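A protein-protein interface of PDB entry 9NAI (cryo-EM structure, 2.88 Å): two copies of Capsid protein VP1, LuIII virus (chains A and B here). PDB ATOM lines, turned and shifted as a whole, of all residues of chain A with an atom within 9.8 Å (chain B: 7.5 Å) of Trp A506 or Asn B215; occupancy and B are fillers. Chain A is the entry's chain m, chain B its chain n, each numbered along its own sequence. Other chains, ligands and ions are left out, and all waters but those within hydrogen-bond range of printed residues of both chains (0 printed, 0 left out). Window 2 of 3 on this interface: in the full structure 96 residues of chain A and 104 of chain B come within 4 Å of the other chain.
N of Phe B210 sits close to ND2 of Asn A507. The backbone NH (N) of Trp A506 sits at hydrogen-bond distance from the backbone carbonyl oxygen (O) of Phe B210, 2.9 Å away.
NE2 of Gln B217 sits close to OG1 of Thr B216 (3.5 Å). O of Thr B212 sits at hydrogen-bond distance from OG1 of Thr B216 (3.0 Å). The side-chain hydroxyl of Thr B216 sits at hydrogen-bond distance from the backbone carbonyl oxygen of Ile B213 (3.2 Å).
Ile B149 touches Ala A504 (CG2 to CB, 3.5 Å). O of Ala A504 touches CD1 of Phe B211, at 3.96 Å. Thr B216 touches Ala A504 (CG2 to O, 3.7 Å). Phe B210 touches Thr A505 (O to CG2, 3.2 Å). OG1 of Thr A505 touches CE1 of Phe B211 (3.5 Å). Trp A506 touches Asn B215 (CE3 to ND2, 3.7 Å). C of Gln B209 touches ND2 of Asn A507, 3.8 Å away.
Printed residues of chain B within 4 Å of Ala A504: Ile B149 (3.5 Å), Phe B211 (3.96 Å) and Thr B216 (3.7 Å). Of the printed residues of chain B, Thr A505 touches Phe B210 and Phe B211. Trp A506 touches just these residues of chain B: Phe B210 and Asn B215. Of the printed residues of chain B, Asn A507 touches Gln B209 and Phe B210. Of the printed residues of chain A, Ile B149 touches Ala A504. Printed residues of chain A within 4 Å of Phe B211: Ala A504 and Thr A505. No residue of chain A comes within 4 Å of Thr B212. Ile B213 touches none of the printed residues of chain A. Of chain A, only Trp A506 comes within 4 Å of Asn B215. Of chain A, only Ala A504 comes within 4 Å of Thr B216. Arg B218 touches none of the printed residues of chain A. The nearest residue of chain A that does not touch Asn B215 is Ala A504 (5.1 Å). The nearest printed residue of chain A that does not touch Phe B211 is Trp A506 (4.9 Å).
Hydrophobic or aromatic side chains of chain A within 4 Å of the printed part of chain B: Ala A504 and Trp A506. Of the 13 printed residues of chain B, 6 touch a printed residue of chain A. Printed residues of chain B that touch a printed residue of chain A: Ile B149, Gln B209, Phe B210, Phe B211, Asn B215 and Thr B216. Hydrophobic or aromatic side chains of chain B within 4 Å of the printed part of chain A: Ile B149, Phe B210 and Phe B211. Among the printed residues, 9 pairs touch across the chains. Among the printed residues, no Asp or Glu carboxylate lies within 4 Å of a Lys or Arg side-chain nitrogen of the other chain.
No position is printed for both chains. Of the 9 pairs that touch across the chains among the printed residues, none has its exchanged pair printed and touching as well.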
ATOM      1  N   ASN A 503     -15.576 -16.970  19.814  1.00  0.00           N
ATOM      2  CA  ASN A 503     -16.630 -16.398  18.984  1.00  0.00           C
ATOM      3  C   ASN A 503     -16.680 -17.131  17.655  1.00  0.00           C
ATOM      4  O   ASN A 503     -15.760 -17.024  16.841  1.00  0.00           O
ATOM      5  CB  ASN A 503     -16.428 -14.898  18.789  1.00  0.00           C
ATOM      6  CG  ASN A 503     -15.102 -14.570  18.171  1.00  0.00           C
ATOM      7  OD1 ASN A 503     -14.200 -15.398  18.143  1.00  0.00           O
ATOM      8  ND2 ASN A 503     -14.974 -13.357  17.664  1.00  0.00           N
ATOM      9  N   ALA A 504     -17.745 -17.885  17.438  1.00  0.00           N
ATOM     10  CA  ALA A 504     -17.982 -18.523  16.158  1.00  0.00           C
ATOM     11  C   ALA A 504     -18.970 -17.772  15.290  1.00  0.00           C
ATOM     12  O   ALA A 504     -19.201 -18.176  14.150  1.00  0.00           O
ATOM     13  CB  ALA A 504     -18.475 -19.947  16.370  1.00  0.00           C
ATOM     14  N   THR A 505     -19.558 -16.702  15.788  1.00  0.00           N
ATOM     15  CA  THR A 505     -20.672 -16.103  15.085  1.00  0.00           C
ATOM     16  C   THR A 505     -20.175 -15.169  13.997  1.00  0.00           C
ATOM     17  O   THR A 505     -19.143 -14.517  14.135  1.00  0.00           O
ATOM     18  CB  THR A 505     -21.561 -15.352  16.063  1.00  0.00           C
ATOM     19  OG1 THR A 505     -22.023 -16.267  17.057  1.00  0.00           O
ATOM     20  CG2 THR A 505     -22.756 -14.801  15.356  1.00  0.00           C
ATOM     21  N   TRP A 506     -20.914 -15.127  12.891  1.00  0.00           N
ATOM     22  CA  TRP A 506     -20.618 -14.161  11.845  1.00  0.00           C
ATOM     23  C   TRP A 506     -20.822 -12.742  12.340  1.00  0.00           C
ATOM     24  O   TRP A 506     -19.953 -11.882  12.177  1.00  0.00           O
ATOM     25  CB  TRP A 506     -21.509 -14.416  10.644  1.00  0.00           C
ATOM     26  CG  TRP A 506     -21.338 -13.426   9.566  1.00  0.00           C
ATOM     27  CD1 TRP A 506     -22.125 -12.357   9.319  1.00  0.00           C
ATOM     28  CD2 TRP A 506     -20.355 -13.447   8.542  1.00  0.00           C
ATOM     29  NE1 TRP A 506     -21.672 -11.679   8.224  1.00  0.00           N
ATOM     30  CE2 TRP A 506     -20.585 -12.336   7.725  1.00  0.00           C
ATOM     31  CE3 TRP A 506     -19.292 -14.291   8.244  1.00  0.00           C
ATOM     32  CZ2 TRP A 506     -19.796 -12.047   6.634  1.00  0.00           C
ATOM     33  CZ3 TRP A 506     -18.511 -14.001   7.164  1.00  0.00           C
ATOM     34  CH2 TRP A 506     -18.764 -12.890   6.370  1.00  0.00           C
ATOM     35  N   ASN A 507     -21.965 -12.479  12.938  1.00  0.00           N
ATOM     36  CA  ASN A 507     -22.348 -11.118  13.241  1.00  0.00           C
ATOM     37  C   ASN A 507     -21.633 -10.616  14.483  1.00  0.00           C
ATOM     38  O   ASN A 507     -21.105 -11.399  15.269  1.00  0.00           O
ATOM     39  CB  ASN A 507     -23.857 -11.042  13.415  1.00  0.00           C
ATOM     40  CG  ASN A 507     -24.359 -11.855  14.583  1.00  0.00           C
ATOM     41  OD1 ASN A 507     -23.736 -11.922  15.632  1.00  0.00           O
ATOM     42  ND2 ASN A 507     -25.488 -12.510  14.390  1.00  0.00           N
ATOM     43  N   PRO A 508     -21.584  -9.308  14.670  1.00  0.00           N
ATOM     44  CA  PRO A 508     -20.997  -8.769  15.892  1.00  0.00           C
ATOM     45  C   PRO A 508     -21.854  -9.061  17.109  1.00  0.00           C
ATOM     46  O   PRO A 508     -23.077  -8.944  17.073  1.00  0.00           O
ATOM     47  CB  PRO A 508     -20.930  -7.270  15.607  1.00  0.00           C
ATOM     48  CG  PRO A 508     -20.840  -7.194  14.147  1.00  0.00           C
ATOM     49  CD  PRO A 508     -21.732  -8.271  13.646  1.00  0.00           C
ATOM     50  N   VAL A 509     -21.197  -9.454  18.189  1.00  0.00           N
ATOM     51  CA  VAL A 509     -21.882  -9.672  19.452  1.00  0.00           C
ATOM     52  C   VAL A 509     -22.119  -8.345  20.160  1.00  0.00           C
ATOM     53  O   VAL A 509     -21.438  -7.348  19.923  1.00  0.00           O
ATOM     54  CB  VAL A 509     -21.099 -10.636  20.347  1.00  0.00           C
ATOM     55  CG1 VAL A 509     -21.019 -11.983  19.697  1.00  0.00           C
ATOM     56  CG2 VAL A 509     -19.725 -10.093  20.598  1.00  0.00           C
ATOM     57  N   TYR B  45     -27.187 -18.463   2.639  1.00  0.00           N
ATOM     58  CA  TYR B  45     -27.848 -18.478   3.929  1.00  0.00           C
ATOM     59  C   TYR B  45     -29.004 -17.496   3.885  1.00  0.00           C
ATOM     60  O   TYR B  45     -28.877 -16.407   3.329  1.00  0.00           O
ATOM     61  CB  TYR B  45     -26.872 -18.105   5.030  1.00  0.00           C
ATOM     62  CG  TYR B  45     -25.776 -19.107   5.224  1.00  0.00           C
ATOM     63  CD1 TYR B  45     -25.948 -20.188   6.060  1.00  0.00           C
ATOM     64  CD2 TYR B  45     -24.571 -18.974   4.575  1.00  0.00           C
ATOM     65  CE1 TYR B  45     -24.955 -21.102   6.248  1.00  0.00           C
ATOM     66  CE2 TYR B  45     -23.572 -19.888   4.756  1.00  0.00           C
ATOM     67  CZ  TYR B  45     -23.768 -20.952   5.596  1.00  0.00           C
ATOM     68  OH  TYR B  45     -22.771 -21.875   5.786  1.00  0.00           O
ATOM     69  N   ILE B 149     -20.523 -26.669  18.020  1.00  0.00           N
ATOM     70  CA  ILE B 149     -20.619 -25.221  17.975  1.00  0.00           C
ATOM     71  C   ILE B 149     -21.938 -24.792  17.364  1.00  0.00           C
ATOM     72  O   ILE B 149     -22.551 -23.815  17.801  1.00  0.00           O
ATOM     73  CB  ILE B 149     -19.426 -24.654  17.203  1.00  0.00           C
ATOM     74  CG1 ILE B 149     -18.142 -24.935  17.968  1.00  0.00           C
ATOM     75  CG2 ILE B 149     -19.598 -23.189  16.995  1.00  0.00           C
ATOM     76  CD1 ILE B 149     -16.907 -24.642  17.179  1.00  0.00           C
ATOM     77  N   GLN B 209     -27.710 -14.623  16.947  1.00  0.00           N
ATOM     78  CA  GLN B 209     -26.585 -15.472  16.585  1.00  0.00           C
ATOM     79  C   GLN B 209     -26.811 -16.000  15.184  1.00  0.00           C
ATOM     80  O   GLN B 209     -27.802 -16.686  14.931  1.00  0.00           O
ATOM     81  CB  GLN B 209     -26.413 -16.636  17.554  1.00  0.00           C
ATOM     82  CG  GLN B 209     -25.959 -16.242  18.923  1.00  0.00           C
ATOM     83  CD  GLN B 209     -25.835 -17.431  19.830  1.00  0.00           C
ATOM     84  OE1 GLN B 209     -26.498 -18.442  19.633  1.00  0.00           O
ATOM     85  NE2 GLN B 209     -24.963 -17.332  20.819  1.00  0.00           N
ATOM     86  N   PHE B 210     -25.897 -15.681  14.282  1.00  0.00           N
ATOM     87  CA  PHE B 210     -25.907 -16.203  12.925  1.00  0.00           C
ATOM     88  C   PHE B 210     -24.627 -16.981  12.688  1.00  0.00           C
ATOM     89  O   PHE B 210     -23.537 -16.404  12.672  1.00  0.00           O
ATOM     90  CB  PHE B 210     -26.074 -15.083  11.909  1.00  0.00           C
ATOM     91  CG  PHE B 210     -25.784 -15.500  10.514  1.00  0.00           C
ATOM     92  CD1 PHE B 210     -26.636 -16.321   9.827  1.00  0.00           C
ATOM     93  CD2 PHE B 210     -24.685 -15.006   9.866  1.00  0.00           C
ATOM     94  CE1 PHE B 210     -26.356 -16.689   8.540  1.00  0.00           C
ATOM     95  CE2 PHE B 210     -24.411 -15.360   8.582  1.00  0.00           C
ATOM     96  CZ  PHE B 210     -25.244 -16.201   7.917  1.00  0.00           C
ATOM     97  N   PHE B 211     -24.765 -18.281  12.496  1.00  0.00           N
ATOM     98  CA  PHE B 211     -23.633 -19.164  12.301  1.00  0.00           C
ATOM     99  C   PHE B 211     -23.533 -19.566  10.844  1.00  0.00           C
ATOM    100  O   PHE B 211     -24.536 -19.671  10.139  1.00  0.00           O
ATOM    101  CB  PHE B 211     -23.753 -20.415  13.157  1.00  0.00           C
ATOM    102  CG  PHE B 211     -23.736 -20.144  14.611  1.00  0.00           C
ATOM    103  CD1 PHE B 211     -22.546 -19.975  15.275  1.00  0.00           C
ATOM    104  CD2 PHE B 211     -24.909 -20.065  15.319  1.00  0.00           C
ATOM    105  CE1 PHE B 211     -22.529 -19.729  16.615  1.00  0.00           C
ATOM    106  CE2 PHE B 211     -24.896 -19.820  16.659  1.00  0.00           C
ATOM    107  CZ  PHE B 211     -23.704 -19.652  17.309  1.00  0.00           C
ATOM    108  N   THR B 212     -22.309 -19.783  10.403  1.00  0.00           N
ATOM    109  CA  THR B 212     -22.020 -20.199   9.046  1.00  0.00           C
ATOM    110  C   THR B 212     -21.168 -21.452   9.073  1.00  0.00           C
ATOM    111  O   THR B 212     -20.170 -21.516   9.790  1.00  0.00           O
ATOM    112  CB  THR B 212     -21.309 -19.097   8.297  1.00  0.00           C
ATOM    113  OG1 THR B 212     -22.189 -17.978   8.166  1.00  0.00           O
ATOM    114  CG2 THR B 212     -20.884 -19.567   6.953  1.00  0.00           C
ATOM    115  N   ILE B 213     -21.577 -22.448   8.294  1.00  0.00           N
ATOM    116  CA  ILE B 213     -20.857 -23.711   8.287  1.00  0.00           C
ATOM    117  C   ILE B 213     -19.402 -23.482   7.932  1.00  0.00           C
ATOM    118  O   ILE B 213     -18.495 -23.993   8.595  1.00  0.00           O
ATOM    119  CB  ILE B 213     -21.515 -24.686   7.304  1.00  0.00           C
ATOM    120  CG1 ILE B 213     -22.992 -24.817   7.625  1.00  0.00           C
ATOM    121  CG2 ILE B 213     -20.854 -26.022   7.397  1.00  0.00           C
ATOM    122  CD1 ILE B 213     -23.258 -25.295   8.988  1.00  0.00           C
ATOM    123  N   GLU B 214     -19.161 -22.693   6.893  1.00  0.00           N
ATOM    124  CA  GLU B 214     -17.809 -22.501   6.390  1.00  0.00           C
ATOM    125  C   GLU B 214     -16.904 -21.870   7.431  1.00  0.00           C
ATOM    126  O   GLU B 214     -15.716 -22.193   7.507  1.00  0.00           O
ATOM    127  CB  GLU B 214     -17.863 -21.651   5.129  1.00  0.00           C
ATOM    128  CG  GLU B 214     -18.493 -22.373   3.961  1.00  0.00           C
ATOM    129  CD  GLU B 214     -20.001 -22.413   4.031  1.00  0.00           C
ATOM    130  OE1 GLU B 214     -20.568 -21.954   5.041  1.00  0.00           O
ATOM    131  OE2 GLU B 214     -20.623 -22.919   3.077  1.00  0.00           O
ATOM    132  N   ASN B 215     -17.433 -20.962   8.235  1.00  0.00           N
ATOM    133  CA  ASN B 215     -16.576 -20.311   9.209  1.00  0.00           C
ATOM    134  C   ASN B 215     -16.342 -21.158  10.445  1.00  0.00           C
ATOM    135  O   ASN B 215     -15.349 -20.955  11.142  1.00  0.00           O
ATOM    136  CB  ASN B 215     -17.165 -18.970   9.597  1.00  0.00           C
ATOM    137  CG  ASN B 215     -17.063 -17.970   8.490  1.00  0.00           C
ATOM    138  OD1 ASN B 215     -16.000 -17.413   8.243  1.00  0.00           O
ATOM    139  ND2 ASN B 215     -18.162 -17.748   7.798  1.00  0.00           N
ATOM    140  N   THR B 216     -17.248 -22.066  10.765  1.00  0.00           N
ATOM    141  CA  THR B 216     -17.154 -22.806  12.010  1.00  0.00           C
ATOM    142  C   THR B 216     -16.534 -24.183  11.877  1.00  0.00           C
ATOM    143  O   THR B 216     -16.339 -24.850  12.892  1.00  0.00           O
ATOM    144  CB  THR B 216     -18.537 -22.952  12.616  1.00  0.00           C
ATOM    145  OG1 THR B 216     -19.372 -23.649  11.688  1.00  0.00           O
ATOM    146  CG2 THR B 216     -19.122 -21.596  12.871  1.00  0.00           C
ATOM    147  N   GLN B 217     -16.213 -24.635  10.673  1.00  0.00           N
ATOM    148  CA  GLN B 217     -15.950 -26.050  10.485  1.00  0.00           C
ATOM    149  C   GLN B 217     -14.758 -26.248   9.571  1.00  0.00           C
ATOM    150  O   GLN B 217     -14.291 -25.318   8.916  1.00  0.00           O
ATOM    151  CB  GLN B 217     -17.161 -26.759   9.890  1.00  0.00           C
ATOM    152  CG  GLN B 217     -18.376 -26.715  10.767  1.00  0.00           C
ATOM    153  CD  GLN B 217     -18.121 -27.321  12.110  1.00  0.00           C
ATOM    154  OE1 GLN B 217     -17.434 -28.331  12.225  1.00  0.00           O
ATOM    155  NE2 GLN B 217     -18.668 -26.707  13.145  1.00  0.00           N
ATOM    156  N   ARG B 218     -14.265 -27.477   9.541  1.00  0.00           N
ATOM    157  CA  ARG B 218     -13.313 -27.905   8.530  1.00  0.00           C
ATOM    158  C   ARG B 218     -14.053 -28.790   7.544  1.00  0.00           C
ATOM    159  O   ARG B 218     -14.576 -29.840   7.924  1.00  0.00           O
ATOM    160  CB  ARG B 218     -12.144 -28.664   9.143  1.00  0.00           C
ATOM    161  CG  ARG B 218     -11.312 -27.841  10.073  1.00  0.00           C
ATOM    162  CD  ARG B 218     -10.192 -28.672  10.632  1.00  0.00           C
ATOM    163  NE  ARG B 218      -9.286 -29.087   9.570  1.00  0.00           N
ATOM    164  CZ  ARG B 218      -8.260 -29.906   9.746  1.00  0.00           C
ATOM    165  NH1 ARG B 218      -8.005 -30.401  10.947  1.00  0.00           N
ATOM    166  NH2 ARG B 218      -7.485 -30.227   8.722  1.00  0.00           N
ATOM    167  N   ILE B 219     -14.101 -28.372   6.293  1.00  0.00           N
ATOM    168  CA  ILE B 219     -14.848 -29.079   5.266  1.00  0.00           C
ATOM    169  C   ILE B 219     -13.894 -29.940   4.461  1.00  0.00           C
ATOM    170  O   ILE B 219     -12.860 -29.461   3.988  1.00  0.00           O
ATOM    171  CB  ILE B 219     -15.602 -28.103   4.356  1.00  0.00           C
ATOM    172  CG1 ILE B 219     -16.714 -27.427   5.142  1.00  0.00           C
ATOM    173  CG2 ILE B 219     -16.172 -28.831   3.176  1.00  0.00           C
ATOM    174  CD1 ILE B 219     -16.358 -26.082   5.657  1.00  0.00           C
